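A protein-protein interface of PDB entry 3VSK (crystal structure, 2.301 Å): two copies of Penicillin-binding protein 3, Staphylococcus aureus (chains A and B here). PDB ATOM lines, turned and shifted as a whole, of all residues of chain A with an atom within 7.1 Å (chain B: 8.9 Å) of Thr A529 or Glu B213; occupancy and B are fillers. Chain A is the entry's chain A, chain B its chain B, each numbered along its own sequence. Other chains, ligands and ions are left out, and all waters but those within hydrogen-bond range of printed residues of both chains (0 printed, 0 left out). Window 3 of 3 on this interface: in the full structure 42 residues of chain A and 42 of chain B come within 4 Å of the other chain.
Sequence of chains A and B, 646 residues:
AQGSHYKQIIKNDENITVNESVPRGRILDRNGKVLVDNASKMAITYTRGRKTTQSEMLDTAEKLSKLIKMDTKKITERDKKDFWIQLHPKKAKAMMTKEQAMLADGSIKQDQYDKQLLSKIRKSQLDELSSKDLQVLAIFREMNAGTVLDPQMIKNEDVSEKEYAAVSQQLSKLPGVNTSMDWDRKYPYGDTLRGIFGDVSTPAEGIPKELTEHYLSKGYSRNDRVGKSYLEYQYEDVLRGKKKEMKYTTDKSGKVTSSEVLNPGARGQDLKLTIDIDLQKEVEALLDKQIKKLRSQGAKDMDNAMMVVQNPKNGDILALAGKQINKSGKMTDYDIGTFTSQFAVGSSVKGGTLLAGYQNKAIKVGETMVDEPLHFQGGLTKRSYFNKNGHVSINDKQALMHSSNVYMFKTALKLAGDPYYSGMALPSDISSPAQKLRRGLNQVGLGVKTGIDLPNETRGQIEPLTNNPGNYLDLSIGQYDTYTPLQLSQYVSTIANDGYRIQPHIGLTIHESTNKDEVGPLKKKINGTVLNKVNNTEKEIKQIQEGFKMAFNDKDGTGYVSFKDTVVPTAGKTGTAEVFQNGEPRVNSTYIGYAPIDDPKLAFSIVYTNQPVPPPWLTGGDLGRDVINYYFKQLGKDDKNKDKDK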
ATOM      1  N   ASN A 314     -11.866  31.875 -11.385  1.00  0.00           N
ATOM      2  CA  ASN A 314     -13.147  32.541 -11.557  1.00  0.00           C
ATOM      3  C   ASN A 314     -13.495  33.004 -12.979  1.00  0.00           C
ATOM      4  O   ASN A 314     -14.402  33.810 -13.160  1.00  0.00           O
ATOM      5  CB  ASN A 314     -13.260  33.699 -10.575  1.00  0.00           C
ATOM      6  CG  ASN A 314     -12.301  34.830 -10.899  1.00  0.00           C
ATOM      7  OD1 ASN A 314     -11.592  34.786 -11.921  1.00  0.00           O
ATOM      8  ND2 ASN A 314     -12.281  35.866 -10.040  1.00  0.00           N
ATOM      9  N   GLY A 315     -12.766  32.510 -13.978  1.00  0.00           N
ATOM     10  CA  GLY A 315     -13.103  32.788 -15.366  1.00  0.00           C
ATOM     11  C   GLY A 315     -12.854  34.211 -15.854  1.00  0.00           C
ATOM     12  O   GLY A 315     -13.163  34.522 -17.002  1.00  0.00           O
ATOM     13  N   THR A 450     -16.518  27.400 -24.691  1.00  0.00           N
ATOM     14  CA  THR A 450     -16.150  27.666 -23.307  1.00  0.00           C
ATOM     15  C   THR A 450     -17.286  28.355 -22.622  1.00  0.00           C
ATOM     16  O   THR A 450     -17.416  28.272 -21.408  1.00  0.00           O
ATOM     17  CB  THR A 450     -14.929  28.582 -23.201  1.00  0.00           C
ATOM     18  OG1 THR A 450     -15.229  29.853 -23.802  1.00  0.00           O
ATOM     19  CG2 THR A 450     -13.708  27.918 -23.855  1.00  0.00           C
ATOM     20  N   GLN A 490      -9.238  27.877 -21.123  1.00  0.00           N
ATOM     21  CA  GLN A 490     -10.197  27.146 -20.298  1.00  0.00           C
ATOM     22  C   GLN A 490      -9.622  25.811 -19.830  1.00  0.00           C
ATOM     23  O   GLN A 490      -9.773  25.444 -18.674  1.00  0.00           O
ATOM     24  CB  GLN A 490     -11.517  26.908 -21.034  1.00  0.00           C
ATOM     25  CG  GLN A 490     -12.550  26.185 -20.183  1.00  0.00           C
ATOM     26  CD  GLN A 490     -13.957  26.253 -20.773  1.00  0.00           C
ATOM     27  OE1 GLN A 490     -14.262  25.585 -21.773  1.00  0.00           O
ATOM     28  NE2 GLN A 490     -14.822  27.063 -20.154  1.00  0.00           N
ATOM     29  N   ARG A 501     -14.068  23.165 -14.258  1.00  0.00           N
ATOM     30  CA  ARG A 501     -14.091  23.923 -15.516  1.00  0.00           C
ATOM     31  C   ARG A 501     -15.085  25.062 -15.381  1.00  0.00           C
ATOM     32  O   ARG A 501     -16.238  24.853 -15.005  1.00  0.00           O
ATOM     33  CB  ARG A 501     -14.441  23.058 -16.741  1.00  0.00           C
ATOM     34  CG  ARG A 501     -14.497  23.874 -18.026  1.00  0.00           C
ATOM     35  CD  ARG A 501     -14.664  23.013 -19.261  1.00  0.00           C
ATOM     36  NE  ARG A 501     -16.061  22.652 -19.476  1.00  0.00           N
ATOM     37  CZ  ARG A 501     -16.842  23.168 -20.428  1.00  0.00           C
ATOM     38  NH1 ARG A 501     -16.368  24.080 -21.273  1.00  0.00           N
ATOM     39  NH2 ARG A 501     -18.096  22.770 -20.537  1.00  0.00           N
ATOM     40  N   ILE A 502     -14.631  26.265 -15.701  1.00  0.00           N
ATOM     41  CA  ILE A 502     -15.387  27.466 -15.407  1.00  0.00           C
ATOM     42  C   ILE A 502     -15.638  28.287 -16.660  1.00  0.00           C
ATOM     43  O   ILE A 502     -14.742  28.494 -17.481  1.00  0.00           O
ATOM     44  CB  ILE A 502     -14.657  28.331 -14.366  1.00  0.00           C
ATOM     45  CG1 ILE A 502     -14.498  27.543 -13.067  1.00  0.00           C
ATOM     46  CG2 ILE A 502     -15.379  29.683 -14.116  1.00  0.00           C
ATOM     47  CD1 ILE A 502     -14.163  28.433 -11.915  1.00  0.00           C
ATOM     48  N   GLN A 503     -16.874  28.755 -16.792  1.00  0.00           N
ATOM     49  CA  GLN A 503     -17.265  29.610 -17.893  1.00  0.00           C
ATOM     50  C   GLN A 503     -16.587  30.982 -17.797  1.00  0.00           C
ATOM     51  O   GLN A 503     -16.974  31.828 -16.991  1.00  0.00           O
ATOM     52  CB  GLN A 503     -18.771  29.799 -17.872  1.00  0.00           C
ATOM     53  CG  GLN A 503     -19.310  30.551 -19.056  1.00  0.00           C
ATOM     54  CD  GLN A 503     -20.820  30.615 -19.028  1.00  0.00           C
ATOM     55  OE1 GLN A 503     -21.492  29.783 -19.634  1.00  0.00           O
ATOM     56  NE2 GLN A 503     -21.362  31.600 -18.311  1.00  0.00           N
ATOM     57  N   PRO A 504     -15.613  31.217 -18.676  1.00  0.00           N
ATOM     58  CA  PRO A 504     -14.845  32.459 -18.659  1.00  0.00           C
ATOM     59  C   PRO A 504     -15.785  33.609 -18.930  1.00  0.00           C
ATOM     60  O   PRO A 504     -16.818  33.403 -19.556  1.00  0.00           O
ATOM     61  CB  PRO A 504     -13.883  32.291 -19.847  1.00  0.00           C
ATOM     62  CG  PRO A 504     -14.569  31.354 -20.766  1.00  0.00           C
ATOM     63  CD  PRO A 504     -15.438  30.459 -19.930  1.00  0.00           C
ATOM     64  N   HIS A 505     -15.448  34.798 -18.452  1.00  0.00           N
ATOM     65  CA  HIS A 505     -16.317  35.937 -18.690  1.00  0.00           C
ATOM     66  C   HIS A 505     -15.524  37.213 -18.748  1.00  0.00           C
ATOM     67  O   HIS A 505     -14.617  37.440 -17.946  1.00  0.00           O
ATOM     68  CB  HIS A 505     -17.392  36.008 -17.624  1.00  0.00           C
ATOM     69  CG  HIS A 505     -16.849  36.012 -16.236  1.00  0.00           C
ATOM     70  ND1 HIS A 505     -16.969  37.099 -15.389  1.00  0.00           N
ATOM     71  CD2 HIS A 505     -16.170  35.070 -15.535  1.00  0.00           C
ATOM     72  CE1 HIS A 505     -16.403  36.819 -14.232  1.00  0.00           C
ATOM     73  NE2 HIS A 505     -15.907  35.592 -14.292  1.00  0.00           N
ATOM     74  N   ILE A 526     -21.478  39.364 -12.516  1.00  0.00           N
ATOM     75  CA  ILE A 526     -21.453  38.378 -13.606  1.00  0.00           C
ATOM     76  C   ILE A 526     -20.481  37.289 -13.156  1.00  0.00           C
ATOM     77  O   ILE A 526     -19.291  37.550 -12.939  1.00  0.00           O
ATOM     78  CB  ILE A 526     -21.041  39.012 -14.979  1.00  0.00           C
ATOM     79  CG1 ILE A 526     -22.098  40.032 -15.406  1.00  0.00           C
ATOM     80  CG2 ILE A 526     -20.884  37.936 -16.066  1.00  0.00           C
ATOM     81  CD1 ILE A 526     -21.702  40.960 -16.545  1.00  0.00           C
ATOM     82  N   ASN A 527     -20.992  36.080 -12.967  1.00  0.00           N
ATOM     83  CA  ASN A 527     -20.203  35.066 -12.275  1.00  0.00           C
ATOM     84  C   ASN A 527     -19.570  34.030 -13.187  1.00  0.00           C
ATOM     85  O   ASN A 527     -20.152  33.660 -14.192  1.00  0.00           O
ATOM     86  CB  ASN A 527     -21.055  34.371 -11.212  1.00  0.00           C
ATOM     87  CG  ASN A 527     -21.333  35.265 -10.009  1.00  0.00           C
ATOM     88  OD1 ASN A 527     -20.548  35.310  -9.054  1.00  0.00           O
ATOM     89  ND2 ASN A 527     -22.452  35.982 -10.051  1.00  0.00           N
ATOM     90  N   GLY A 528     -18.381  33.557 -12.808  1.00  0.00           N
ATOM     91  CA  GLY A 528     -17.742  32.433 -13.464  1.00  0.00           C
ATOM     92  C   GLY A 528     -18.449  31.152 -13.061  1.00  0.00           C
ATOM     93  O   GLY A 528     -18.089  30.502 -12.087  1.00  0.00           O
ATOM     94  N   THR A 529     -19.468  30.782 -13.820  1.00  0.00           N
ATOM     95  CA  THR A 529     -20.238  29.589 -13.512  1.00  0.00           C
ATOM     96  C   THR A 529     -19.371  28.342 -13.655  1.00  0.00           C
ATOM     97  O   THR A 529     -18.598  28.238 -14.605  1.00  0.00           O
ATOM     98  CB  THR A 529     -21.416  29.479 -14.469  1.00  0.00           C
ATOM     99  OG1 THR A 529     -22.113  30.735 -14.505  1.00  0.00           O
ATOM    100  CG2 THR A 529     -22.354  28.332 -14.040  1.00  0.00           C
ATOM    101  N   VAL A 530     -19.466  27.408 -12.714  1.00  0.00           N
ATOM    102  CA  VAL A 530     -18.803  26.114 -12.886  1.00  0.00           C
ATOM    103  C   VAL A 530     -19.589  25.299 -13.902  1.00  0.00           C
ATOM    104  O   VAL A 530     -20.768  25.038 -13.717  1.00  0.00           O
ATOM    105  CB  VAL A 530     -18.703  25.320 -11.559  1.00  0.00           C
ATOM    106  CG1 VAL A 530     -18.657  23.809 -11.836  1.00  0.00           C
ATOM    107  CG2 VAL A 530     -17.484  25.750 -10.752  1.00  0.00           C
ATOM    108  N   LEU A 531     -18.952  24.910 -14.999  1.00  0.00           N
ATOM    109  CA  LEU A 531     -19.673  24.163 -16.020  1.00  0.00           C
ATOM    110  C   LEU A 531     -19.713  22.664 -15.696  1.00  0.00           C
ATOM    111  O   LEU A 531     -20.662  21.966 -16.055  1.00  0.00           O
ATOM    112  CB  LEU A 531     -19.027  24.349 -17.380  1.00  0.00           C
ATOM    113  CG  LEU A 531     -19.301  25.548 -18.277  1.00  0.00           C
ATOM    114  CD1 LEU A 531     -20.224  26.585 -17.654  1.00  0.00           C
ATOM    115  CD2 LEU A 531     -17.946  26.131 -18.650  1.00  0.00           C
ATOM    116  N   ASN A 532     -18.666  22.178 -15.033  1.00  0.00           N
ATOM    117  CA  ASN A 532     -18.555  20.775 -14.632  1.00  0.00           C
ATOM    118  C   ASN A 532     -17.199  20.508 -13.986  1.00  0.00           C
ATOM    119  O   ASN A 532     -16.313  21.373 -14.005  1.00  0.00           O
ATOM    120  CB  ASN A 532     -18.726  19.827 -15.824  1.00  0.00           C
ATOM    121  CG  ASN A 532     -17.542  19.858 -16.787  1.00  0.00           C
ATOM    122  OD1 ASN A 532     -17.564  20.570 -17.805  1.00  0.00           O
ATOM    123  ND2 ASN A 532     -16.504  19.069 -16.480  1.00  0.00           N
ATOM    124  N   ILE B 207     -27.432  12.818 -16.862  1.00  0.00           N
ATOM    125  CA  ILE B 207     -26.907  13.990 -17.556  1.00  0.00           C
ATOM    126  C   ILE B 207     -25.431  13.767 -17.804  1.00  0.00           C
ATOM    127  O   ILE B 207     -24.677  13.480 -16.863  1.00  0.00           O
ATOM    128  CB  ILE B 207     -27.052  15.260 -16.731  1.00  0.00           C
ATOM    129  CG1 ILE B 207     -28.490  15.753 -16.797  1.00  0.00           C
ATOM    130  CG2 ILE B 207     -26.098  16.359 -17.240  1.00  0.00           C
ATOM    131  CD1 ILE B 207     -28.839  16.646 -15.620  1.00  0.00           C
ATOM    132  N   PRO B 208     -24.996  13.915 -19.070  1.00  0.00           N
ATOM    133  CA  PRO B 208     -23.578  13.679 -19.378  1.00  0.00           C
ATOM    134  C   PRO B 208     -22.731  14.798 -18.765  1.00  0.00           C
ATOM    135  O   PRO B 208     -23.128  15.974 -18.899  1.00  0.00           O
ATOM    136  CB  PRO B 208     -23.525  13.728 -20.916  1.00  0.00           C
ATOM    137  CG  PRO B 208     -24.971  13.772 -21.368  1.00  0.00           C
ATOM    138  CD  PRO B 208     -25.742  14.385 -20.247  1.00  0.00           C
ATOM    139  N   LYS B 209     -21.607  14.440 -18.126  1.00  0.00           N
ATOM    140  CA  LYS B 209     -20.910  15.332 -17.194  1.00  0.00           C
ATOM    141  C   LYS B 209     -20.633  16.699 -17.802  1.00  0.00           C
ATOM    142  O   LYS B 209     -20.786  17.727 -17.121  1.00  0.00           O
ATOM    143  CB  LYS B 209     -19.619  14.696 -16.640  1.00  0.00           C
ATOM    144  CG  LYS B 209     -18.905  15.514 -15.518  1.00  0.00           C
ATOM    145  CD  LYS B 209     -19.524  15.286 -14.130  1.00  0.00           C
ATOM    146  CE  LYS B 209     -18.951  16.219 -13.049  1.00  0.00           C
ATOM    147  NZ  LYS B 209     -19.458  17.649 -13.073  1.00  0.00           N
ATOM    148  N   GLU B 210     -20.254  16.710 -19.077  1.00  0.00           N
ATOM    149  CA  GLU B 210     -20.018  17.970 -19.782  1.00  0.00           C
ATOM    150  C   GLU B 210     -21.223  18.908 -19.721  1.00  0.00           C
ATOM    151  O   GLU B 210     -21.044  20.115 -19.563  1.00  0.00           O
ATOM    152  CB  GLU B 210     -19.607  17.716 -21.232  1.00  0.00           C
ATOM    153  CG  GLU B 210     -19.915  16.312 -21.714  1.00  0.00           C
ATOM    154  CD  GLU B 210     -20.646  16.310 -23.034  1.00  0.00           C
ATOM    155  OE1 GLU B 210     -20.551  17.332 -23.751  1.00  0.00           O
ATOM    156  OE2 GLU B 210     -21.321  15.299 -23.346  1.00  0.00           O
ATOM    157  N   LEU B 211     -22.437  18.355 -19.824  1.00  0.00           N
ATOM    158  CA  LEU B 211     -23.649  19.171 -19.871  1.00  0.00           C
ATOM    159  C   LEU B 211     -24.240  19.443 -18.492  1.00  0.00           C
ATOM    160  O   LEU B 211     -25.370  19.917 -18.395  1.00  0.00           O
ATOM    161  CB  LEU B 211     -24.729  18.538 -20.768  1.00  0.00           C
ATOM    162  CG  LEU B 211     -24.367  18.295 -22.238  1.00  0.00           C
ATOM    163  CD1 LEU B 211     -25.456  17.522 -22.924  1.00  0.00           C
ATOM    164  CD2 LEU B 211     -24.076  19.610 -22.982  1.00  0.00           C
ATOM    165  N   THR B 212     -23.497  19.149 -17.425  1.00  0.00           N
ATOM    166  CA  THR B 212     -24.061  19.262 -16.068  1.00  0.00           C
ATOM    167  C   THR B 212     -24.845  20.574 -15.772  1.00  0.00           C
ATOM    168  O   THR B 212     -26.028  20.548 -15.391  1.00  0.00           O
ATOM    169  CB  THR B 212     -22.989  19.066 -14.984  1.00  0.00           C
ATOM    170  OG1 THR B 212     -22.302  17.828 -15.210  1.00  0.00           O
ATOM    171  CG2 THR B 212     -23.635  19.063 -13.583  1.00  0.00           C
ATOM    172  N   GLU B 213     -24.190  21.715 -15.958  1.00  0.00           N
ATOM    173  CA  GLU B 213     -24.809  22.978 -15.597  1.00  0.00           C
ATOM    174  C   GLU B 213     -25.915  23.336 -16.584  1.00  0.00           C
ATOM    175  O   GLU B 213     -26.881  24.017 -16.236  1.00  0.00           O
ATOM    176  CB  GLU B 213     -23.751  24.083 -15.539  1.00  0.00           C
ATOM    177  CG  GLU B 213     -24.209  25.342 -14.809  1.00  0.00           C
ATOM    178  CD  GLU B 213     -24.818  26.379 -15.737  1.00  0.00           C
ATOM    179  OE1 GLU B 213     -24.811  26.151 -16.964  1.00  0.00           O
ATOM    180  OE2 GLU B 213     -25.304  27.428 -15.248  1.00  0.00           O
ATOM    181  N   HIS B 214     -25.784  22.866 -17.818  1.00  0.00           N
ATOM    182  CA  HIS B 214     -26.752  23.204 -18.835  1.00  0.00           C
ATOM    183  C   HIS B 214     -28.081  22.594 -18.505  1.00  0.00           C
ATOM    184  O   HIS B 214     -29.117  23.154 -18.842  1.00  0.00           O
ATOM    185  CB  HIS B 214     -26.346  22.702 -20.208  1.00  0.00           C
ATOM    186  CG  HIS B 214     -27.422  22.880 -21.227  1.00  0.00           C
ATOM    187  ND1 HIS B 214     -28.220  21.840 -21.661  1.00  0.00           N
ATOM    188  CD2 HIS B 214     -27.882  23.991 -21.847  1.00  0.00           C
ATOM    189  CE1 HIS B 214     -29.099  22.300 -22.532  1.00  0.00           C
ATOM    190  NE2 HIS B 214     -28.913  23.603 -22.666  1.00  0.00           N
ATOM    191  N   TYR B 215     -28.049  21.432 -17.864  1.00  0.00           N
ATOM    192  CA  TYR B 215     -29.283  20.735 -17.547  1.00  0.00           C
ATOM    193  C   TYR B 215     -29.691  20.871 -16.073  1.00  0.00           C
ATOM    194  O   TYR B 215     -30.883  21.006 -15.785  1.00  0.00           O
ATOM    195  CB  TYR B 215     -29.225  19.269 -18.022  1.00  0.00           C
ATOM    196  CG  TYR B 215     -29.596  19.059 -19.489  1.00  0.00           C
ATOM    197  CD1 TYR B 215     -30.759  19.598 -20.022  1.00  0.00           C
ATOM    198  CD2 TYR B 215     -28.771  18.324 -20.339  1.00  0.00           C
ATOM    199  CE1 TYR B 215     -31.096  19.408 -21.381  1.00  0.00           C
ATOM    200  CE2 TYR B 215     -29.095  18.129 -21.684  1.00  0.00           C
ATOM    201  CZ  TYR B 215     -30.265  18.670 -22.202  1.00  0.00           C
ATOM    202  OH  TYR B 215     -30.579  18.464 -23.535  1.00  0.00           O
ATOM    203  N   LEU B 216     -28.747  20.845 -15.128  1.00  0.00           N
ATOM    204  CA  LEU B 216     -29.122  21.201 -13.722  1.00  0.00           C
ATOM    205  C   LEU B 216     -29.727  22.593 -13.590  1.00  0.00           C
ATOM    206  O   LEU B 216     -30.490  22.853 -12.671  1.00  0.00           O
ATOM    207  CB  LEU B 216     -27.951  21.097 -12.747  1.00  0.00           C
ATOM    208  CG  LEU B 216     -27.907  19.815 -11.932  1.00  0.00           C
ATOM    209  CD1 LEU B 216     -28.439  18.664 -12.770  1.00  0.00           C
ATOM    210  CD2 LEU B 216     -26.479  19.528 -11.469  1.00  0.00           C
ATOM    211  N   SER B 217     -29.389  23.490 -14.509  1.00  0.00           N
ATOM    212  CA  SER B 217     -29.957  24.829 -14.471  1.00  0.00           C
ATOM    213  C   SER B 217     -31.449  24.769 -14.759  1.00  0.00           C
ATOM    214  O   SER B 217     -32.185  25.728 -14.495  1.00  0.00           O
ATOM    215  CB  SER B 217     -29.248  25.751 -15.474  1.00  0.00           C
ATOM    216  OG  SER B 217     -29.063  25.100 -16.723  1.00  0.00           O
ATOM    217  N   LYS B 218     -31.884  23.624 -15.280  1.00  0.00           N
ATOM    218  CA  LYS B 218     -33.240  23.451 -15.794  1.00  0.00           C
ATOM    219  C   LYS B 218     -34.137  22.592 -14.887  1.00  0.00           C
ATOM    220  O   LYS B 218     -35.222  22.156 -15.297  1.00  0.00           O
ATOM    221  CB  LYS B 218     -33.189  22.827 -17.195  1.00  0.00           C
ATOM    222  CG  LYS B 218     -32.167  23.432 -18.138  1.00  0.00           C
ATOM    223  CD  LYS B 218     -32.797  24.490 -19.026  1.00  0.00           C
ATOM    224  CE  LYS B 218     -31.931  24.762 -20.243  1.00  0.00           C
ATOM    225  NZ  LYS B 218     -31.789  23.524 -21.059  1.00  0.00           N
ATOM    226  N   GLY B 219     -33.687  22.345 -13.663  1.00  0.00           N
ATOM    227  CA  GLY B 219     -34.478  21.577 -12.719  1.00  0.00           C
ATOM    228  C   GLY B 219     -34.355  20.080 -12.916  1.00  0.00           C
ATOM    229  O   GLY B 219     -35.026  19.302 -12.218  1.00  0.00           O
ATOM    230  N   TYR B 220     -33.509  19.667 -13.867  1.00  0.00           N
ATOM    231  CA  TYR B 220     -33.201  18.241 -14.066  1.00  0.00           C
ATOM    232  C   TYR B 220     -32.409  17.683 -12.879  1.00  0.00           C
ATOM    233  O   TYR B 220     -31.869  18.432 -12.064  1.00  0.00           O
ATOM    234  CB  TYR B 220     -32.391  18.013 -15.354  1.00  0.00           C
ATOM    235  CG  TYR B 220     -33.154  18.141 -16.667  1.00  0.00           C
ATOM    236  CD1 TYR B 220     -33.454  19.391 -17.197  1.00  0.00           C
ATOM    237  CD2 TYR B 220     -33.539  17.013 -17.399  1.00  0.00           C
ATOM    238  CE1 TYR B 220     -34.136  19.522 -18.410  1.00  0.00           C
ATOM    239  CE2 TYR B 220     -34.218  17.136 -18.633  1.00  0.00           C
ATOM    240  CZ  TYR B 220     -34.511  18.399 -19.125  1.00  0.00           C
ATOM    241  OH  TYR B 220     -35.182  18.571 -20.319  1.00  0.00           O
ATOM    242  N   TYR B 233     -31.217  17.159 -28.672  1.00  0.00           N
ATOM    243  CA  TYR B 233     -30.783  18.230 -27.780  1.00  0.00           C
ATOM    244  C   TYR B 233     -31.535  19.554 -28.030  1.00  0.00           C
ATOM    245  O   TYR B 233     -31.829  20.306 -27.102  1.00  0.00           O
ATOM    246  CB  TYR B 233     -29.256  18.424 -27.939  1.00  0.00           C
ATOM    247  CG  TYR B 233     -28.693  19.564 -27.141  1.00  0.00           C
ATOM    248  CD1 TYR B 233     -28.547  20.821 -27.712  1.00  0.00           C
ATOM    249  CD2 TYR B 233     -28.336  19.396 -25.806  1.00  0.00           C
ATOM    250  CE1 TYR B 233     -28.028  21.886 -26.986  1.00  0.00           C
ATOM    251  CE2 TYR B 233     -27.831  20.456 -25.060  1.00  0.00           C
ATOM    252  CZ  TYR B 233     -27.670  21.699 -25.659  1.00  0.00           C
ATOM    253  OH  TYR B 233     -27.165  22.762 -24.927  1.00  0.00           O
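Among the printed residues, pairs that only touch across the chains: Asn A532 with Lys B209 (3.2 Å), Thr A529 with Glu B213 (3.3 Å), Leu A531 with Glu B213 (3.5 Å), Val A530 with Glu B213 (3.6 Å), Leu A531 with Thr B212 (3.9 Å), Asn A532 with Glu B210 (3.9 Å) and Leu A531 with Glu B210 (3.98 Å).
The backbone NH (N) of Leu A531 is in hydrogen-bond range of the backbone carbonyl oxygen (O) of Arg A501 (2.7 Å).
N of Arg A501 sits at hydrogen-bond distance from O of Asn A532, 2.9 Å away.
The backbone NH (N) of Gln A503 lies within hydrogen-bond range of the backbone carbonyl oxygen (O) of Thr A529 (2.8 Å).
O of Lys B209 sits at hydrogen-bond distance from OG1 of Thr B212 (2.4 Å).
The backbone carbonyl oxygen (O) of Glu B213 is in hydrogen-bond range of the side-chain hydroxyl (OG) of Ser B217 (2.5 Å).
Thr A529 touches just one residue of chain B: Glu B213.
Of chain A, only Thr A529, Val A530 and Leu A531 come within 4 Å of Glu B213.
No residue of chain B comes within 4 Å of Gly A528.
Printed residues of chain A within 4 Å of Glu B210: Leu A531 (3.98 Å) and Asn A532 (3.9 Å).
Of the printed residues of chain A, Thr B212 touches Leu A531 (3.9 Å).
Of the printed residues of chain B, Val A530 touches Glu B213 (3.6 Å).
Of the printed residues of chain B, Leu A531 touches Glu B210 (3.98 Å), Thr B212 (3.9 Å) and Glu B213 (3.5 Å).
Of the printed residues of chain B, Asn A532 touches Lys B209 and Glu B210.
Gln A503 touches none of the printed residues of chain B.
His B214 touches none of the printed residues of chain A.
The nearest residue of chain A that does not touch Glu B213 is Asn A532 (5.5 Å).
The nearest printed residue of chain B that does not touch Asn A532 is Thr B212 (4.1 Å).
No position is printed for both chains.
Of the 16 printed residues of chain A, 4 touch a printed residue of chain B.
Printed residues of chain B that touch a printed residue of chain A: Lys B209, Glu B210, Thr B212 and Glu B213.
Among the printed residues, no Asp or Glu carboxylate lies within 4 Å of a Lys or Arg side-chain nitrogen of the other chain.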
